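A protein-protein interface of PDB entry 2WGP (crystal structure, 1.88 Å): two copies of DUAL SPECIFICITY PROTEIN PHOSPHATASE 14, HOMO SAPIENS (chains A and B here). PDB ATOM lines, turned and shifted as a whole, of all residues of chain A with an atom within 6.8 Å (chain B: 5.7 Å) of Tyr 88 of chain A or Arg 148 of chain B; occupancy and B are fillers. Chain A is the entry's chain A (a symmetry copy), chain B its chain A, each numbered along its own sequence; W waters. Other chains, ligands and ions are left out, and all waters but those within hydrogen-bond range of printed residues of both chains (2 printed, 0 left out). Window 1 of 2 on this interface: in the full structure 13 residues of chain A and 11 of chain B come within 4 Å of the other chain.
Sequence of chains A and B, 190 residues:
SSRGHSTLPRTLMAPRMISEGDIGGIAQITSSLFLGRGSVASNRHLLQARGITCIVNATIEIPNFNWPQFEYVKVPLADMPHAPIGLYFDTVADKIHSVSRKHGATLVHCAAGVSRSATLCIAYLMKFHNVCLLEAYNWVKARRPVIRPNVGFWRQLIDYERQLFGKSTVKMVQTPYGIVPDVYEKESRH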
ATOM      1  N   ILE A  60       8.368  23.455   2.805  1.00  0.00           N
ATOM      2  CA  ILE A  60       9.003  22.335   2.157  1.00  0.00           C
ATOM      3  C   ILE A  60       8.449  22.205   0.725  1.00  0.00           C
ATOM      4  O   ILE A  60       9.197  21.943  -0.217  1.00  0.00           O
ATOM      5  CB  ILE A  60       8.843  21.050   3.032  1.00  0.00           C
ATOM      6  CG1 ILE A  60       9.527  19.833   2.397  1.00  0.00           C
ATOM      7  CG2 ILE A  60       7.370  20.748   3.345  1.00  0.00           C
ATOM      8  CD1 ILE A  60       9.751  18.729   3.397  1.00  0.00           C
ATOM      9  N   LYS A  74      15.691  28.931   1.859  1.00  0.00           N
ATOM     10  CA  LYS A  74      14.681  27.885   2.038  1.00  0.00           C
ATOM     11  C   LYS A  74      14.715  27.408   3.487  1.00  0.00           C
ATOM     12  O   LYS A  74      15.775  27.034   3.999  1.00  0.00           O
ATOM     13  CB  LYS A  74      15.008  26.731   1.104  1.00  0.00           C
ATOM     14  CG  LYS A  74      14.107  25.498   1.170  1.00  0.00           C
ATOM     15  CD  LYS A  74      12.882  25.691   0.282  1.00  0.00           C
ATOM     16  CE  LYS A  74      12.321  24.360  -0.156  1.00  0.00           C
ATOM     17  NZ  LYS A  74      11.227  24.516  -1.133  1.00  0.00           N
ATOM     18  N   VAL A  75      13.552  27.429   4.131  1.00  0.00           N
ATOM     19  CA  VAL A  75      13.335  26.890   5.472  1.00  0.00           C
ATOM     20  C   VAL A  75      12.305  25.738   5.337  1.00  0.00           C
ATOM     21  O   VAL A  75      11.092  25.971   5.393  1.00  0.00           O
ATOM     22  CB  VAL A  75      12.848  28.020   6.418  1.00  0.00           C
ATOM     23  CG1 VAL A  75      12.430  27.491   7.795  1.00  0.00           C
ATOM     24  CG2 VAL A  75      13.936  29.099   6.519  1.00  0.00           C
ATOM     25  N   PRO A  76      12.796  24.495   5.156  1.00  0.00           N
ATOM     26  CA  PRO A  76      11.910  23.442   4.669  1.00  0.00           C
ATOM     27  C   PRO A  76      11.135  22.731   5.774  1.00  0.00           C
ATOM     28  O   PRO A  76      11.413  21.559   6.100  1.00  0.00           O
ATOM     29  CB  PRO A  76      12.868  22.495   3.929  1.00  0.00           C
ATOM     30  CG  PRO A  76      14.137  22.631   4.626  1.00  0.00           C
ATOM     31  CD  PRO A  76      14.209  24.050   5.133  1.00  0.00           C
ATOM     32  N   LEU A  77      10.093  23.416   6.235  1.00  0.00           N
ATOM     33  CA  LEU A  77       9.189  22.972   7.286  1.00  0.00           C
ATOM     34  C   LEU A  77       7.778  22.749   6.745  1.00  0.00           C
ATOM     35  O   LEU A  77       7.358  23.438   5.831  1.00  0.00           O
ATOM     36  CB  LEU A  77       9.030  24.103   8.322  1.00  0.00           C
ATOM     37  CG  LEU A  77      10.243  24.575   9.115  1.00  0.00           C
ATOM     38  CD1 LEU A  77      10.005  26.042   9.591  1.00  0.00           C
ATOM     39  CD2 LEU A  77      10.518  23.623  10.265  1.00  0.00           C
ATOM     40  N   PRO A  84       9.786  21.527  14.040  1.00  0.00           N
ATOM     41  CA  PRO A  84      10.649  22.286  14.960  1.00  0.00           C
ATOM     42  C   PRO A  84      11.061  23.639  14.382  1.00  0.00           C
ATOM     43  O   PRO A  84      12.266  23.932  14.218  1.00  0.00           O
ATOM     44  CB  PRO A  84      11.866  21.356  15.130  1.00  0.00           C
ATOM     45  CG  PRO A  84      11.983  20.715  13.805  1.00  0.00           C
ATOM     46  CD  PRO A  84      10.565  20.501  13.311  1.00  0.00           C
ATOM     47  N   ILE A  85      10.050  24.463  14.112  1.00  0.00           N
ATOM     48  CA  ILE A  85      10.225  25.796  13.539  1.00  0.00           C
ATOM     49  C   ILE A  85      11.149  26.704  14.384  1.00  0.00           C
ATOM     50  O   ILE A  85      11.889  27.541  13.843  1.00  0.00           O
ATOM     51  CB  ILE A  85       8.855  26.468  13.295  1.00  0.00           C
ATOM     52  CG1 ILE A  85       8.999  27.757  12.480  1.00  0.00           C
ATOM     53  CG2 ILE A  85       8.147  26.792  14.628  1.00  0.00           C
ATOM     54  CD1 ILE A  85       7.687  28.213  11.847  1.00  0.00           C
ATOM     55  N   GLY A  86      11.125  26.515  15.695  1.00  0.00           N
ATOM     56  CA  GLY A  86      11.983  27.243  16.602  1.00  0.00           C
ATOM     57  C   GLY A  86      13.474  27.179  16.301  1.00  0.00           C
ATOM     58  O   GLY A  86      14.226  28.091  16.670  1.00  0.00           O
ATOM     59  N   LEU A  87      13.904  26.105  15.637  1.00  0.00           N
ATOM     60  CA  LEU A  87      15.297  25.941  15.252  1.00  0.00           C
ATOM     61  C   LEU A  87      15.707  26.980  14.203  1.00  0.00           C
ATOM     62  O   LEU A  87      16.889  27.138  13.918  1.00  0.00           O
ATOM     63  CB  LEU A  87      15.549  24.513  14.722  1.00  0.00           C
ATOM     64  CG  LEU A  87      15.478  23.325  15.696  1.00  0.00           C
ATOM     65  CD1 LEU A  87      15.676  21.960  14.993  1.00  0.00           C
ATOM     66  CD2 LEU A  87      16.500  23.466  16.825  1.00  0.00           C
ATOM     67  N   TYR A  88      14.728  27.655  13.609  1.00  0.00           N
ATOM     68  CA  TYR A  88      14.970  28.709  12.632  1.00  0.00           C
ATOM     69  C   TYR A  88      14.718  30.120  13.177  1.00  0.00           C
ATOM     70  O   TYR A  88      14.864  31.101  12.448  1.00  0.00           O
ATOM     71  CB  TYR A  88      14.127  28.469  11.388  1.00  0.00           C
ATOM     72  CG  TYR A  88      14.507  27.203  10.623  1.00  0.00           C
ATOM     73  CD1 TYR A  88      15.546  27.215   9.688  1.00  0.00           C
ATOM     74  CD2 TYR A  88      13.845  26.008  10.843  1.00  0.00           C
ATOM     75  CE1 TYR A  88      15.894  26.073   8.965  1.00  0.00           C
ATOM     76  CE2 TYR A  88      14.193  24.848  10.115  1.00  0.00           C
ATOM     77  CZ  TYR A  88      15.228  24.896   9.189  1.00  0.00           C
ATOM     78  OH  TYR A  88      15.601  23.769   8.468  1.00  0.00           O
ATOM     79  N   PHE A  89      14.330  30.238  14.448  1.00  0.00           N
ATOM     80  CA  PHE A  89      13.986  31.548  15.001  1.00  0.00           C
ATOM     81  C   PHE A  89      15.172  32.510  14.896  1.00  0.00           C
ATOM     82  O   PHE A  89      15.039  33.584  14.283  1.00  0.00           O
ATOM     83  CB  PHE A  89      13.493  31.445  16.450  1.00  0.00           C
ATOM     84  CG  PHE A  89      12.062  30.907  16.615  1.00  0.00           C
ATOM     85  CD1 PHE A  89      11.599  30.590  17.895  1.00  0.00           C
ATOM     86  CD2 PHE A  89      11.177  30.718  15.529  1.00  0.00           C
ATOM     87  CE1 PHE A  89      10.303  30.109  18.077  1.00  0.00           C
ATOM     88  CE2 PHE A  89       9.896  30.237  15.737  1.00  0.00           C
ATOM     89  CZ  PHE A  89       9.468  29.944  17.001  1.00  0.00           C
ATOM     90  N   ASP A  90      16.325  32.114  15.443  1.00  0.00           N
ATOM     91  CA  ASP A  90      17.529  32.963  15.433  1.00  0.00           C
ATOM     92  C   ASP A  90      18.072  33.136  14.017  1.00  0.00           C
ATOM     93  O   ASP A  90      18.366  34.243  13.601  1.00  0.00           O
ATOM     94  CB  ASP A  90      18.637  32.407  16.353  1.00  0.00           C
ATOM     95  CG  ASP A  90      18.348  32.651  17.829  1.00  0.00           C
ATOM     96  OD1 ASP A  90      18.602  31.738  18.655  1.00  0.00           O
ATOM     97  OD2 ASP A  90      17.872  33.758  18.168  1.00  0.00           O
ATOM     98  N   THR A  91      18.156  32.047  13.251  1.00  0.00           N
ATOM     99  CA  THR A  91      18.786  32.143  11.934  1.00  0.00           C
ATOM    100  C   THR A  91      17.971  33.008  10.965  1.00  0.00           C
ATOM    101  O   THR A  91      18.550  33.844  10.242  1.00  0.00           O
ATOM    102  CB  THR A  91      19.138  30.753  11.358  1.00  0.00           C
ATOM    103  OG1 THR A  91      17.954  29.987  11.194  1.00  0.00           O
ATOM    104  CG2 THR A  91      20.102  29.990  12.317  1.00  0.00           C
ATOM    105  N   VAL A  92      16.639  32.889  10.981  1.00  0.00           N
ATOM    106  CA  VAL A  92      15.797  33.700  10.090  1.00  0.00           C
ATOM    107  C   VAL A  92      15.750  35.148  10.591  1.00  0.00           C
ATOM    108  O   VAL A  92      15.830  36.082   9.792  1.00  0.00           O
ATOM    109  CB  VAL A  92      14.358  33.106   9.858  1.00  0.00           C
ATOM    110  CG1 VAL A  92      13.430  34.076   9.124  1.00  0.00           C
ATOM    111  CG2 VAL A  92      14.437  31.771   9.082  1.00  0.00           C
ATOM    112  N   ALA A  93      15.588  35.327  11.904  1.00  0.00           N
ATOM    113  CA  ALA A  93      15.573  36.657  12.498  1.00  0.00           C
ATOM    114  C   ALA A  93      16.897  37.396  12.226  1.00  0.00           C
ATOM    115  O   ALA A  93      16.895  38.564  11.835  1.00  0.00           O
ATOM    116  CB  ALA A  93      15.276  36.567  13.987  1.00  0.00           C
ATOM    117  N   ASP A  94      18.013  36.705  12.396  1.00  0.00           N
ATOM    118  CA  ASP A  94      19.332  37.260  12.048  1.00  0.00           C
ATOM    119  C   ASP A  94      19.458  37.637  10.559  1.00  0.00           C
ATOM    120  O   ASP A  94      20.042  38.665  10.233  1.00  0.00           O
ATOM    121  CB  ASP A  94      20.443  36.286  12.445  1.00  0.00           C
ATOM    122  CG  ASP A  94      20.595  36.147  13.946  1.00  0.00           C
ATOM    123  OD1 ASP A  94      19.918  36.884  14.701  1.00  0.00           O
ATOM    124  OD2 ASP A  94      21.415  35.302  14.371  1.00  0.00           O
ATOM    125  N   LEU A 120       7.634  32.999  12.230  1.00  0.00           N
ATOM    126  CA  LEU A 120       8.985  33.502  12.057  1.00  0.00           C
ATOM    127  C   LEU A 120       9.067  35.022  12.176  1.00  0.00           C
ATOM    128  O   LEU A 120      10.024  35.544  12.777  1.00  0.00           O
ATOM    129  CB  LEU A 120       9.543  33.031  10.714  1.00  0.00           C
ATOM    130  CG  LEU A 120       9.759  31.514  10.568  1.00  0.00           C
ATOM    131  CD1 LEU A 120      10.066  31.181   9.120  1.00  0.00           C
ATOM    132  CD2 LEU A 120      10.859  31.000  11.552  1.00  0.00           C
ATOM    133  N   ALA A 123       8.806  35.916  15.860  1.00  0.00           N
ATOM    134  CA  ALA A 123      10.072  35.650  16.541  1.00  0.00           C
ATOM    135  C   ALA A 123      11.072  36.796  16.269  1.00  0.00           C
ATOM    136  O   ALA A 123      11.749  37.268  17.191  1.00  0.00           O
ATOM    137  CB  ALA A 123      10.643  34.291  16.102  1.00  0.00           C
ATOM    138  N   VAL B 114      13.435  16.977  -0.594  1.00  0.00           N
ATOM    139  CA  VAL B 114      13.909  17.389   0.719  1.00  0.00           C
ATOM    140  C   VAL B 114      14.096  16.224   1.732  1.00  0.00           C
ATOM    141  O   VAL B 114      15.096  16.166   2.465  1.00  0.00           O
ATOM    142  CB  VAL B 114      12.929  18.477   1.294  1.00  0.00           C
ATOM    143  CG1 VAL B 114      13.165  18.743   2.766  1.00  0.00           C
ATOM    144  CG2 VAL B 114      13.053  19.776   0.516  1.00  0.00           C
ATOM    145  N   SER B 115      13.118  15.317   1.796  1.00  0.00           N
ATOM    146  CA  SER B 115      13.018  14.348   2.886  1.00  0.00           C
ATOM    147  C   SER B 115      13.041  12.880   2.409  1.00  0.00           C
ATOM    148  O   SER B 115      14.022  12.173   2.654  1.00  0.00           O
ATOM    149  CB  SER B 115      11.780  14.648   3.736  1.00  0.00           C
ATOM    150  OG  SER B 115      11.608  13.699   4.784  1.00  0.00           O
ATOM    151  N   ALA B 118      16.068  12.114  -0.183  1.00  0.00           N
ATOM    152  CA  ALA B 118      17.340  12.332   0.529  1.00  0.00           C
ATOM    153  C   ALA B 118      17.602  11.199   1.489  1.00  0.00           C
ATOM    154  O   ALA B 118      18.745  10.750   1.627  1.00  0.00           O
ATOM    155  CB  ALA B 118      17.300  13.671   1.313  1.00  0.00           C
ATOM    156  N   TYR B 137      25.008  12.237   5.257  1.00  0.00           N
ATOM    157  CA  TYR B 137      24.246  13.490   5.345  1.00  0.00           C
ATOM    158  C   TYR B 137      25.009  14.668   4.752  1.00  0.00           C
ATOM    159  O   TYR B 137      24.487  15.365   3.875  1.00  0.00           O
ATOM    160  CB  TYR B 137      23.825  13.735   6.808  1.00  0.00           C
ATOM    161  CG  TYR B 137      23.118  15.045   7.046  1.00  0.00           C
ATOM    162  CD1 TYR B 137      21.834  15.282   6.544  1.00  0.00           C
ATOM    163  CD2 TYR B 137      23.745  16.045   7.770  1.00  0.00           C
ATOM    164  CE1 TYR B 137      21.197  16.525   6.776  1.00  0.00           C
ATOM    165  CE2 TYR B 137      23.125  17.255   8.017  1.00  0.00           C
ATOM    166  CZ  TYR B 137      21.866  17.491   7.530  1.00  0.00           C
ATOM    167  OH  TYR B 137      21.288  18.713   7.790  1.00  0.00           O
ATOM    168  N   LYS B 141      23.924  16.858   1.572  1.00  0.00           N
ATOM    169  CA  LYS B 141      23.715  18.269   1.933  1.00  0.00           C
ATOM    170  C   LYS B 141      24.683  19.210   1.156  1.00  0.00           C
ATOM    171  O   LYS B 141      24.297  20.319   0.792  1.00  0.00           O
ATOM    172  CB  LYS B 141      23.811  18.407   3.469  1.00  0.00           C
ATOM    173  CG  LYS B 141      23.512  19.762   4.089  1.00  0.00           C
ATOM    174  CD  LYS B 141      22.059  19.979   4.433  1.00  0.00           C
ATOM    175  CE  LYS B 141      21.913  21.202   5.338  1.00  0.00           C
ATOM    176  NZ  LYS B 141      20.685  21.962   5.100  1.00  0.00           N
ATOM    177  N   VAL B 146      19.086  22.072   0.606  1.00  0.00           N
ATOM    178  CA  VAL B 146      17.731  22.120   1.140  1.00  0.00           C
ATOM    179  C   VAL B 146      17.262  20.821   1.800  1.00  0.00           C
ATOM    180  O   VAL B 146      16.192  20.823   2.414  1.00  0.00           O
ATOM    181  CB  VAL B 146      16.679  22.542   0.063  1.00  0.00           C
ATOM    182  CG1 VAL B 146      17.011  23.935  -0.507  1.00  0.00           C
ATOM    183  CG2 VAL B 146      16.544  21.483  -1.014  1.00  0.00           C
ATOM    184  N   ILE B 147      18.058  19.737   1.733  1.00  0.00           N
ATOM    185  CA  ILE B 147      17.597  18.471   2.330  1.00  0.00           C
ATOM    186  C   ILE B 147      17.350  18.596   3.828  1.00  0.00           C
ATOM    187  O   ILE B 147      18.032  19.358   4.552  1.00  0.00           O
ATOM    188  CB  ILE B 147      18.470  17.213   1.998  1.00  0.00           C
ATOM    189  CG1 ILE B 147      19.860  17.212   2.679  1.00  0.00           C
ATOM    190  CG2 ILE B 147      18.542  17.016   0.476  1.00  0.00           C
ATOM    191  CD1 ILE B 147      20.314  15.798   3.104  1.00  0.00           C
ATOM    192  N   ARG B 148      16.341  17.870   4.267  1.00  0.00           N
ATOM    193  CA  ARG B 148      15.845  17.924   5.645  1.00  0.00           C
ATOM    194  C   ARG B 148      14.922  16.721   5.918  1.00  0.00           C
ATOM    195  O   ARG B 148      13.713  16.857   6.000  1.00  0.00           O
ATOM    196  CB  ARG B 148      15.098  19.242   5.867  1.00  0.00           C
ATOM    197  CG  ARG B 148      14.820  19.560   7.305  1.00  0.00           C
ATOM    198  CD  ARG B 148      15.908  20.348   7.931  1.00  0.00           C
ATOM    199  NE  ARG B 148      15.573  20.755   9.281  1.00  0.00           N
ATOM    200  CZ  ARG B 148      16.383  21.424  10.098  1.00  0.00           C
ATOM    201  NH1 ARG B 148      17.610  21.716   9.722  1.00  0.00           N
ATOM    202  NH2 ARG B 148      15.945  21.799  11.304  1.00  0.00           N
ATOM    203  N   PRO B 149      15.507  15.523   6.057  1.00  0.00           N
ATOM    204  CA  PRO B 149      14.700  14.358   6.401  1.00  0.00           C
ATOM    205  C   PRO B 149      13.899  14.614   7.660  1.00  0.00           C
ATOM    206  O   PRO B 149      14.342  15.344   8.566  1.00  0.00           O
ATOM    207  CB  PRO B 149      15.746  13.280   6.647  1.00  0.00           C
ATOM    208  CG  PRO B 149      16.886  13.671   5.744  1.00  0.00           C
ATOM    209  CD  PRO B 149      16.925  15.168   5.868  1.00  0.00           C
ATOM    210  N   ASN B 150      12.687  14.091   7.710  1.00  0.00           N
ATOM    211  CA  ASN B 150      11.864  14.354   8.869  1.00  0.00           C
ATOM    212  C   ASN B 150      12.433  13.609  10.087  1.00  0.00           C
ATOM    213  O   ASN B 150      13.316  12.790   9.926  1.00  0.00           O
ATOM    214  CB  ASN B 150      10.385  14.079   8.578  1.00  0.00           C
ATOM    215  CG  ASN B 150      10.041  12.616   8.536  1.00  0.00           C
ATOM    216  OD1 ASN B 150      10.345  11.863   9.457  1.00  0.00           O
ATOM    217  ND2 ASN B 150       9.333  12.217   7.491  1.00  0.00           N
ATOM    218  N   TRP B 154      15.046  10.243  10.399  1.00  0.00           N
ATOM    219  CA  TRP B 154      16.285  10.268  11.172  1.00  0.00           C
ATOM    220  C   TRP B 154      16.419   9.104  12.166  1.00  0.00           C
ATOM    221  O   TRP B 154      17.460   8.464  12.188  1.00  0.00           O
ATOM    222  CB  TRP B 154      16.492  11.624  11.866  1.00  0.00           C
ATOM    223  CG  TRP B 154      17.181  12.590  10.967  1.00  0.00           C
ATOM    224  CD1 TRP B 154      16.628  13.652  10.341  1.00  0.00           C
ATOM    225  CD2 TRP B 154      18.559  12.562  10.580  1.00  0.00           C
ATOM    226  NE1 TRP B 154      17.568  14.304   9.588  1.00  0.00           N
ATOM    227  CE2 TRP B 154      18.765  13.650   9.707  1.00  0.00           C
ATOM    228  CE3 TRP B 154      19.641  11.717  10.880  1.00  0.00           C
ATOM    229  CZ2 TRP B 154      20.013  13.931   9.135  1.00  0.00           C
ATOM    230  CZ3 TRP B 154      20.888  12.013  10.321  1.00  0.00           C
ATOM    231  CH2 TRP B 154      21.057  13.108   9.461  1.00  0.00           C
ATOM    232  N   TYR B 184      20.735  19.036  13.395  1.00  0.00           N
ATOM    233  CA  TYR B 184      19.773  20.140  13.277  1.00  0.00           C
ATOM    234  C   TYR B 184      19.960  21.141  14.413  1.00  0.00           C
ATOM    235  O   TYR B 184      19.837  22.344  14.216  1.00  0.00           O
ATOM    236  CB  TYR B 184      18.336  19.639  13.295  1.00  0.00           C
ATOM    237  CG  TYR B 184      17.865  18.904  12.045  1.00  0.00           C
ATOM    238  CD1 TYR B 184      18.716  18.667  10.956  1.00  0.00           C
ATOM    239  CD2 TYR B 184      16.553  18.429  11.968  1.00  0.00           C
ATOM    240  CE1 TYR B 184      18.275  17.980   9.847  1.00  0.00           C
ATOM    241  CE2 TYR B 184      16.103  17.749  10.883  1.00  0.00           C
ATOM    242  CZ  TYR B 184      16.966  17.513   9.808  1.00  0.00           C
ATOM    243  OH  TYR B 184      16.519  16.840   8.689  1.00  0.00           O
ATOM    244  N   GLU B 187      23.190  23.102  13.582  1.00  0.00           N
ATOM    245  CA  GLU B 187      22.872  24.066  12.524  1.00  0.00           C
ATOM    246  C   GLU B 187      22.135  25.332  13.039  1.00  0.00           C
ATOM    247  O   GLU B 187      22.373  26.425  12.522  1.00  0.00           O
ATOM    248  CB  GLU B 187      22.026  23.394  11.414  1.00  0.00           C
ATOM    249  CG  GLU B 187      22.831  22.405  10.523  1.00  0.00           C
ATOM    250  CD  GLU B 187      21.949  21.512   9.648  1.00  0.00           C
ATOM    251  OE1 GLU B 187      22.431  20.446   9.197  1.00  0.00           O
ATOM    252  OE2 GLU B 187      20.779  21.897   9.417  1.00  0.00           O
ATOM    253  N   SER B 188      21.270  25.166  14.043  1.00  0.00           N
ATOM    254  CA  SER B 188      20.444  26.256  14.619  1.00  0.00           C
ATOM    255  C   SER B 188      21.270  27.311  15.368  1.00  0.00           C
ATOM    256  O   SER B 188      20.798  28.426  15.609  1.00  0.00           O
ATOM    257  CB  SER B 188      19.360  25.713  15.567  1.00  0.00           C
ATOM    258  OG  SER B 188      19.892  25.294  16.818  1.00  0.00           O
HETATM  259  O   HOH W   1      18.264  29.353  14.843  1.00  0.00           O
HETATM  260  O   HOH W   2      20.470  29.561  18.272  1.00  0.00           O
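The side-chain hydroxyl of Tyr 88 of chain A sits close to the guanidinium group of Arg 148 of chain B.
Water W1 lies within hydrogen-bond range of O of Leu 87 of chain A (2.8 Å), O of Ser 188 of chain B (2.8 Å), N of Thr 91 of chain A (3.1 Å) and N of Asp 90 of chain A (3.4 Å). Water W2 lies within hydrogen-bond range of the side-chain carboxylate of Asp 90 of chain A (2.9 Å) and the backbone carbonyl oxygen of Ser 188 of chain B (2.9 Å).
The backbone carbonyl oxygen (O) of Leu 77 of chain A sits at hydrogen-bond distance from the backbone NH (N) of Ile 60 of chain A (3.2 Å). N of Arg 148 of chain B is in hydrogen-bond range of O of Val 114 of chain B (2.8 Å). The guanidinium group (NH1) of Arg 148 of chain B lies within salt-bridge range of the side-chain carboxylate (OE2) of Glu 187 of chain B (3.2 Å). OH of Tyr 184 of chain B is in hydrogen-bond range of NE1 of Trp 154 of chain B. The backbone carbonyl oxygen of Ile 60 of chain A is in hydrogen-bond range of the side-chain amino group of Lys 74 of chain A. O of Pro 149 of chain B sits at hydrogen-bond distance from OH of Tyr 184 of chain B.
No position is printed for both chains. Of the 10 pairs that touch across the chains among the printed residues, none has its exchanged pair printed and touching as well.
Among the printed residues, merely in contact across the chains: Leu 87 of chain A with Ser 188 of chain B (3.3 Å), Ile 60 of chain A with Val 114 of chain B (3.5 Å), Pro 76 of chain A with Val 146 of chain B (3.5 Å), Lys 74 of chain A with Val 146 of chain B (3.7 Å), Leu 87 of chain A with Arg 148 of chain B (3.7 Å), Thr 91 of chain A with Ser 188 of chain B (3.7 Å), Pro 76 of chain A with Arg 148 of chain B (3.7 Å), Leu 87 of chain A with Tyr 184 of chain B (3.9 Å) and Pro 76 of chain A with Val 114 of chain B (3.9 Å).
Of the 14 printed residues of chain B, 5 touch a printed residue of chain A. Printed residues of chain B that touch a printed residue of chain A: Val 114, Val 146, Arg 148, Tyr 184 and Ser 188. Hydrophobic or aromatic side chains of chain B that line the printed part of chain A: Val 114, Val 146 and Tyr 184. Printed residues of chain A that touch a printed residue of chain B: Ile 60, Lys 74, Pro 76, Leu 87, Tyr 88 and Thr 91. Among the printed residues, 10 pairs touch across the chains. Among the printed residues, no Asp or Glu carboxylate lies within 4 Å of a Lys or Arg side-chain nitrogen of the other chain.
Printed residues of chain B within 4 Å of Pro 76 of chain A: Val 114 (3.9 Å), Val 146 (3.5 Å) and Arg 148 (3.7 Å). Gly 86 of chain A touches none of the printed residues of chain B. Of chain B, only Arg 148 (3.0 Å) comes within 4 Å of Tyr 88 of chain A. Of the printed residues of chain B, Thr 91 of chain A touches Ser 188. Leu 120 of chain A touches none of the printed residues of chain B. Of the printed residues of chain A, Val 114 of chain B touches Ile 60 and Pro 76. Of chain A, only Pro 76 (3.7 Å), Leu 87 (3.7 Å) and Tyr 88 (3.0 Å) come within 4 Å of Arg 148 of chain B. Of the printed residues of chain A, Tyr 184 of chain B touches Leu 87. Printed residues of chain A within 4 Å of Ser 188 of chain B: Leu 87 and Thr 91. The nearest residue of chain A that does not touch Arg 148 of chain B is Pro 84 of chain A (4.8 Å).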
